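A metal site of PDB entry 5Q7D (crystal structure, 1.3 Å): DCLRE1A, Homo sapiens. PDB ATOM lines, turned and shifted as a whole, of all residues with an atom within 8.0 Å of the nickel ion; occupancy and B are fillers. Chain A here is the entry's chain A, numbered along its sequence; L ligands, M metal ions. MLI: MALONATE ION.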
ATOM      1  N   ASP A  18      -8.512 -31.240 -13.237  1.00  0.00           N
ATOM      2  CA  ASP A  18      -7.186 -30.627 -13.469  1.00  0.00           C
ATOM      3  C   ASP A  18      -5.996 -31.665 -13.255  1.00  0.00           C
ATOM      4  O   ASP A  18      -4.927 -31.346 -12.642  1.00  0.00           O
ATOM      5  CB  ASP A  18      -6.979 -29.321 -12.740  1.00  0.00           C
ATOM      6  CG  ASP A  18      -8.061 -28.235 -13.061  1.00  0.00           C
ATOM      7  OD1 ASP A  18      -8.737 -28.397 -14.101  1.00  0.00           O
ATOM      8  OD2 ASP A  18      -8.088 -27.256 -12.290  1.00  0.00           O
ATOM      9  N   THR A  34     -10.814 -26.958 -15.357  1.00  0.00           N
ATOM     10  CA  THR A  34     -11.445 -25.728 -14.853  1.00  0.00           C
ATOM     11  C   THR A  34     -11.123 -24.499 -15.726  1.00  0.00           C
ATOM     12  O   THR A  34     -12.009 -23.630 -15.879  1.00  0.00           O
ATOM     13  CB  THR A  34     -11.107 -25.439 -13.378  1.00  0.00           C
ATOM     14  OG1 THR A  34      -9.669 -25.235 -13.238  1.00  0.00           O
ATOM     15  CG2 THR A  34     -11.634 -26.548 -12.418  1.00  0.00           C
ATOM     16  N   HIS A  35      -9.884 -24.425 -16.276  1.00  0.00           N
ATOM     17  CA  HIS A  35      -9.439 -23.243 -17.018  1.00  0.00           C
ATOM     18  C   HIS A  35      -8.175 -23.548 -17.776  1.00  0.00           C
ATOM     19  O   HIS A  35      -7.413 -24.451 -17.355  1.00  0.00           O
ATOM     20  CB  HIS A  35      -9.345 -21.966 -16.129  1.00  0.00           C
ATOM     21  CG  HIS A  35      -8.281 -21.964 -15.070  1.00  0.00           C
ATOM     22  ND1 HIS A  35      -8.244 -22.818 -13.963  1.00  0.00           N
ATOM     23  CD2 HIS A  35      -7.145 -21.207 -14.962  1.00  0.00           C
ATOM     24  CE1 HIS A  35      -7.196 -22.479 -13.220  1.00  0.00           C
ATOM     25  NE2 HIS A  35      -6.548 -21.497 -13.782  1.00  0.00           N
ATOM     26  N   PHE A  36      -7.927 -22.683 -18.764  1.00  0.00           N
ATOM     27  CA  PHE A  36      -6.679 -22.848 -19.627  1.00  0.00           C
ATOM     28  C   PHE A  36      -5.456 -22.119 -19.069  1.00  0.00           C
ATOM     29  O   PHE A  36      -4.983 -21.095 -19.696  1.00  0.00           O
ATOM     30  CB  PHE A  36      -7.045 -22.395 -21.088  1.00  0.00           C
ATOM     31  CG  PHE A  36      -6.032 -22.831 -22.138  1.00  0.00           C
ATOM     32  CD1 PHE A  36      -6.042 -24.145 -22.588  1.00  0.00           C
ATOM     33  CD2 PHE A  36      -5.105 -21.937 -22.687  1.00  0.00           C
ATOM     34  CE1 PHE A  36      -5.128 -24.565 -23.557  1.00  0.00           C
ATOM     35  CE2 PHE A  36      -4.202 -22.339 -23.676  1.00  0.00           C
ATOM     36  CZ  PHE A  36      -4.219 -23.617 -24.114  1.00  0.00           C
ATOM     37  N   HIS A  37      -4.941 -22.536 -17.903  1.00  0.00           N
ATOM     38  CA  HIS A  37      -3.632 -22.122 -17.373  1.00  0.00           C
ATOM     39  C   HIS A  37      -2.738 -23.386 -17.289  1.00  0.00           C
ATOM     40  O   HIS A  37      -3.193 -24.505 -16.917  1.00  0.00           O
ATOM     41  CB  HIS A  37      -3.717 -21.429 -15.988  1.00  0.00           C
ATOM     42  CG  HIS A  37      -4.143 -19.965 -16.026  1.00  0.00           C
ATOM     43  ND1 HIS A  37      -4.561 -19.269 -14.915  1.00  0.00           N
ATOM     44  CD2 HIS A  37      -4.118 -19.060 -17.044  1.00  0.00           C
ATOM     45  CE1 HIS A  37      -4.807 -18.006 -15.237  1.00  0.00           C
ATOM     46  NE2 HIS A  37      -4.509 -17.856 -16.518  1.00  0.00           N
ATOM     47  N   SER A  38      -1.448 -23.191 -17.607  1.00  0.00           N
ATOM     48  CA  SER A  38      -0.538 -24.331 -17.857  1.00  0.00           C
ATOM     49  C   SER A  38      -0.360 -25.248 -16.659  1.00  0.00           C
ATOM     50  O   SER A  38      -0.253 -26.469 -16.911  1.00  0.00           O
ATOM     51  CB  SER A  38       0.780 -23.843 -18.489  1.00  0.00           C
ATOM     52  OG  SER A  38       1.478 -22.978 -17.613  1.00  0.00           O
ATOM     53  N   ASP A  39      -0.367 -24.765 -15.428  1.00  0.00           N
ATOM     54  CA  ASP A  39      -0.225 -25.664 -14.233  1.00  0.00           C
ATOM     55  C   ASP A  39      -1.435 -26.624 -14.177  1.00  0.00           C
ATOM     56  O   ASP A  39      -1.327 -27.744 -13.640  1.00  0.00           O
ATOM     57  CB  ASP A  39      -0.096 -24.884 -12.943  1.00  0.00           C
ATOM     58  CG  ASP A  39       1.351 -24.310 -12.673  1.00  0.00           C
ATOM     59  OD1 ASP A  39       2.259 -24.555 -13.482  1.00  0.00           O
ATOM     60  OD2 ASP A  39       1.485 -23.607 -11.639  1.00  0.00           O
ATOM     61  N   HIS A  40      -2.602 -26.197 -14.712  1.00  0.00           N
ATOM     62  CA  HIS A  40      -3.822 -27.024 -14.721  1.00  0.00           C
ATOM     63  C   HIS A  40      -4.022 -27.891 -15.911  1.00  0.00           C
ATOM     64  O   HIS A  40      -4.501 -29.068 -15.735  1.00  0.00           O
ATOM     65  CB  HIS A  40      -5.046 -26.035 -14.488  1.00  0.00           C
ATOM     66  CG  HIS A  40      -4.929 -25.304 -13.203  1.00  0.00           C
ATOM     67  ND1 HIS A  40      -5.659 -25.617 -12.062  1.00  0.00           N
ATOM     68  CD2 HIS A  40      -4.198 -24.216 -12.856  1.00  0.00           C
ATOM     69  CE1 HIS A  40      -5.311 -24.821 -11.083  1.00  0.00           C
ATOM     70  NE2 HIS A  40      -4.433 -23.945 -11.537  1.00  0.00           N
ATOM     71  N   HIS A  96     -12.173 -15.589 -12.723  1.00  0.00           N
ATOM     72  CA  HIS A  96     -10.691 -15.779 -12.840  1.00  0.00           C
ATOM     73  C   HIS A  96     -10.354 -15.281 -14.241  1.00  0.00           C
ATOM     74  O   HIS A  96     -10.503 -14.031 -14.443  1.00  0.00           O
ATOM     75  CB  HIS A  96     -10.348 -17.216 -12.557  1.00  0.00           C
ATOM     76  CG  HIS A  96      -8.868 -17.589 -12.482  1.00  0.00           C
ATOM     77  ND1 HIS A  96      -7.959 -16.864 -11.754  1.00  0.00           N
ATOM     78  CD2 HIS A  96      -8.140 -18.503 -13.172  1.00  0.00           C
ATOM     79  CE1 HIS A  96      -6.743 -17.413 -11.915  1.00  0.00           C
ATOM     80  NE2 HIS A  96      -6.821 -18.414 -12.757  1.00  0.00           N
ATOM     81  N   CYS A  97      -9.804 -16.061 -15.122  1.00  0.00           N
ATOM     82  CA  CYS A  97      -9.493 -15.694 -16.542  1.00  0.00           C
ATOM     83  C   CYS A  97     -10.655 -16.094 -17.470  1.00  0.00           C
ATOM     84  O   CYS A  97     -11.571 -16.795 -17.041  1.00  0.00           O
ATOM     85  CB  CYS A  97      -8.163 -16.393 -16.961  1.00  0.00           C
ATOM     86  SG  CYS A  97      -8.284 -18.227 -16.985  1.00  0.00           S
ATOM     87  N   ALA A 100     -12.848 -19.640 -17.308  1.00  0.00           N
ATOM     88  CA  ALA A 100     -12.627 -20.309 -16.013  1.00  0.00           C
ATOM     89  C   ALA A 100     -13.976 -20.569 -15.312  1.00  0.00           C
ATOM     90  O   ALA A 100     -14.803 -19.674 -15.206  1.00  0.00           O
ATOM     91  CB  ALA A 100     -11.697 -19.518 -15.148  1.00  0.00           C
ATOM     92  N   GLY A 117     -11.985 -24.476  -8.656  1.00  0.00           N
ATOM     93  CA  GLY A 117     -10.855 -24.210  -9.519  1.00  0.00           C
ATOM     94  C   GLY A 117     -10.060 -23.072  -8.961  1.00  0.00           C
ATOM     95  O   GLY A 117      -9.883 -22.958  -7.772  1.00  0.00           O
ATOM     96  N   ASP A 118      -9.495 -22.273  -9.872  1.00  0.00           N
ATOM     97  CA  ASP A 118      -8.954 -20.947  -9.471  1.00  0.00           C
ATOM     98  C   ASP A 118     -10.095 -19.901  -9.549  1.00  0.00           C
ATOM     99  O   ASP A 118     -10.872 -19.867 -10.528  1.00  0.00           O
ATOM    100  CB  ASP A 118      -7.785 -20.479 -10.320  1.00  0.00           C
ATOM    101  CG  ASP A 118      -6.468 -21.148 -10.065  1.00  0.00           C
ATOM    102  OD1 ASP A 118      -6.303 -21.841  -9.067  1.00  0.00           O
ATOM    103  OD2 ASP A 118      -5.542 -20.860 -10.865  1.00  0.00           O
ATOM    104  N   PHE A 119     -10.230 -19.040  -8.523  1.00  0.00           N
ATOM    105  CA  PHE A 119     -11.336 -18.043  -8.480  1.00  0.00           C
ATOM    106  C   PHE A 119     -10.987 -16.768  -7.768  1.00  0.00           C
ATOM    107  O   PHE A 119     -10.111 -16.771  -6.898  1.00  0.00           O
ATOM    108  CB  PHE A 119     -12.705 -18.676  -7.940  1.00  0.00           C
ATOM    109  CG  PHE A 119     -12.960 -18.717  -6.388  1.00  0.00           C
ATOM    110  CD1 PHE A 119     -14.251 -18.441  -5.896  1.00  0.00           C
ATOM    111  CD2 PHE A 119     -11.922 -19.076  -5.480  1.00  0.00           C
ATOM    112  CE1 PHE A 119     -14.493 -18.557  -4.557  1.00  0.00           C
ATOM    113  CE2 PHE A 119     -12.185 -19.162  -4.112  1.00  0.00           C
ATOM    114  CZ  PHE A 119     -13.465 -18.896  -3.680  1.00  0.00           C
ATOM    115  N   ASP A 141      -9.607 -22.798  -3.723  1.00  0.00           N
ATOM    116  CA  ASP A 141      -8.374 -22.058  -4.139  1.00  0.00           C
ATOM    117  C   ASP A 141      -7.979 -21.135  -2.988  1.00  0.00           C
ATOM    118  O   ASP A 141      -8.534 -20.061  -2.716  1.00  0.00           O
ATOM    119  CB  ASP A 141      -8.707 -21.197  -5.395  1.00  0.00           C
ATOM    120  CG  ASP A 141      -7.626 -20.182  -5.752  1.00  0.00           C
ATOM    121  OD1 ASP A 141      -6.516 -20.299  -5.167  1.00  0.00           O
ATOM    122  OD2 ASP A 141      -7.982 -19.276  -6.556  1.00  0.00           O
ATOM    123  N   THR A 143      -4.859 -19.712  -2.693  1.00  0.00           N
ATOM    124  CA  THR A 143      -3.610 -19.027  -3.080  1.00  0.00           C
ATOM    125  C   THR A 143      -3.250 -17.925  -2.115  1.00  0.00           C
ATOM    126  O   THR A 143      -2.061 -17.891  -1.645  1.00  0.00           O
ATOM    127  CB  THR A 143      -3.815 -18.395  -4.527  1.00  0.00           C
ATOM    128  OG1 THR A 143      -3.985 -19.405  -5.520  1.00  0.00           O
ATOM    129  CG2 THR A 143      -2.595 -17.614  -4.963  1.00  0.00           C
ATOM    130  N   SER A 183       0.126 -15.536 -20.236  1.00  0.00           N
ATOM    131  CA  SER A 183      -1.005 -16.461 -20.121  1.00  0.00           C
ATOM    132  C   SER A 183      -2.265 -15.664 -20.475  1.00  0.00           C
ATOM    133  O   SER A 183      -2.247 -14.408 -20.501  1.00  0.00           O
ATOM    134  CB  SER A 183      -1.167 -17.023 -18.657  1.00  0.00           C
ATOM    135  OG  SER A 183      -1.420 -15.940 -17.761  1.00  0.00           O
ATOM    136  N   ILE A 184      -3.363 -16.347 -20.626  1.00  0.00           N
ATOM    137  CA  ILE A 184      -4.643 -15.660 -20.656  1.00  0.00           C
ATOM    138  C   ILE A 184      -5.013 -15.146 -19.258  1.00  0.00           C
ATOM    139  O   ILE A 184      -4.407 -15.558 -18.244  1.00  0.00           O
ATOM    140  CB  ILE A 184      -5.838 -16.515 -21.197  1.00  0.00           C
ATOM    141  CG1 ILE A 184      -6.221 -17.683 -20.308  1.00  0.00           C
ATOM    142  CG2 ILE A 184      -5.567 -16.921 -22.660  1.00  0.00           C
ATOM    143  CD1 ILE A 184      -7.526 -18.340 -20.639  1.00  0.00           C
ATOM    144  N   GLU A 296      -6.469 -11.833 -10.148  1.00  0.00           N
ATOM    145  CA  GLU A 296      -7.577 -12.764 -10.534  1.00  0.00           C
ATOM    146  C   GLU A 296      -7.775 -13.942  -9.526  1.00  0.00           C
ATOM    147  O   GLU A 296      -8.429 -14.950  -9.812  1.00  0.00           O
ATOM    148  CB  GLU A 296      -7.509 -13.244 -11.980  1.00  0.00           C
ATOM    149  CG  GLU A 296      -7.729 -12.036 -13.007  1.00  0.00           C
ATOM    150  CD  GLU A 296      -7.777 -12.416 -14.479  1.00  0.00           C
ATOM    151  OE1 GLU A 296      -7.265 -13.503 -14.857  1.00  0.00           O
ATOM    152  OE2 GLU A 296      -8.324 -11.586 -15.295  1.00  0.00           O
ATOM    153  N   HIS A 297      -7.209 -13.732  -8.334  1.00  0.00           N
ATOM    154  CA  HIS A 297      -7.488 -14.611  -7.158  1.00  0.00           C
ATOM    155  C   HIS A 297      -8.067 -13.823  -5.987  1.00  0.00           C
ATOM    156  O   HIS A 297      -7.789 -12.618  -5.819  1.00  0.00           O
ATOM    157  CB  HIS A 297      -6.212 -15.351  -6.659  1.00  0.00           C
ATOM    158  CG  HIS A 297      -5.582 -16.304  -7.631  1.00  0.00           C
ATOM    159  ND1 HIS A 297      -5.955 -17.649  -7.715  1.00  0.00           N
ATOM    160  CD2 HIS A 297      -4.489 -16.180  -8.444  1.00  0.00           C
ATOM    161  CE1 HIS A 297      -5.200 -18.257  -8.618  1.00  0.00           C
ATOM    162  NE2 HIS A 297      -4.337 -17.387  -9.054  1.00  0.00           N
HETATM  163  C1  MLI L   1      -1.827 -19.386 -12.613  1.00  0.00           C
HETATM  164  C2  MLI L   1      -2.666 -18.425 -11.761  1.00  0.00           C
HETATM  165  C3  MLI L   1      -2.276 -20.860 -12.499  1.00  0.00           C
HETATM  166  O6  MLI L   1      -2.233 -17.595 -10.973  1.00  0.00           O
HETATM  167  O7  MLI L   1      -3.868 -18.521 -11.862  1.00  0.00           O
HETATM  168  O8  MLI L   1      -3.444 -21.213 -12.741  1.00  0.00           O
HETATM  169  O9  MLI L   1      -1.418 -21.778 -12.271  1.00  0.00           O
HETATM  170 NI    NI M   1      -5.156 -19.997 -12.857  1.00  0.00          NI
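The side-chain carboxylate (OD2) of Asp 118 lies close to a ring nitrogen (NE2) of His 40 (3.3 Å). OG1 of Thr 34 is in hydrogen-bond range of ND1 of His 35 (2.9 Å). NE2 of His 37 sits at hydrogen-bond distance from O of Ile 184 (2.9 Å). O of Glu 296 is in hydrogen-bond range of ND1 of His 96.
O8 of the ligand is bound to the nickel ion (2.1 Å). O7 of the ligand binds the nickel ion, at 2.2 Å. OD2 of Asp 118 is bound to the nickel ion, 2.2 Å away. The nickel ion is bound by NE2 of His 35, at 2.2 Å. The nickel ion is bound by a ring nitrogen (ND1) of His 37 (2.3 Å). The nickel ion is bound by a ring nitrogen (NE2) of His 96, 2.3 Å away.
Within 4 Å of the nickel ion: His 35, His 37, His 96 and Asp 118.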
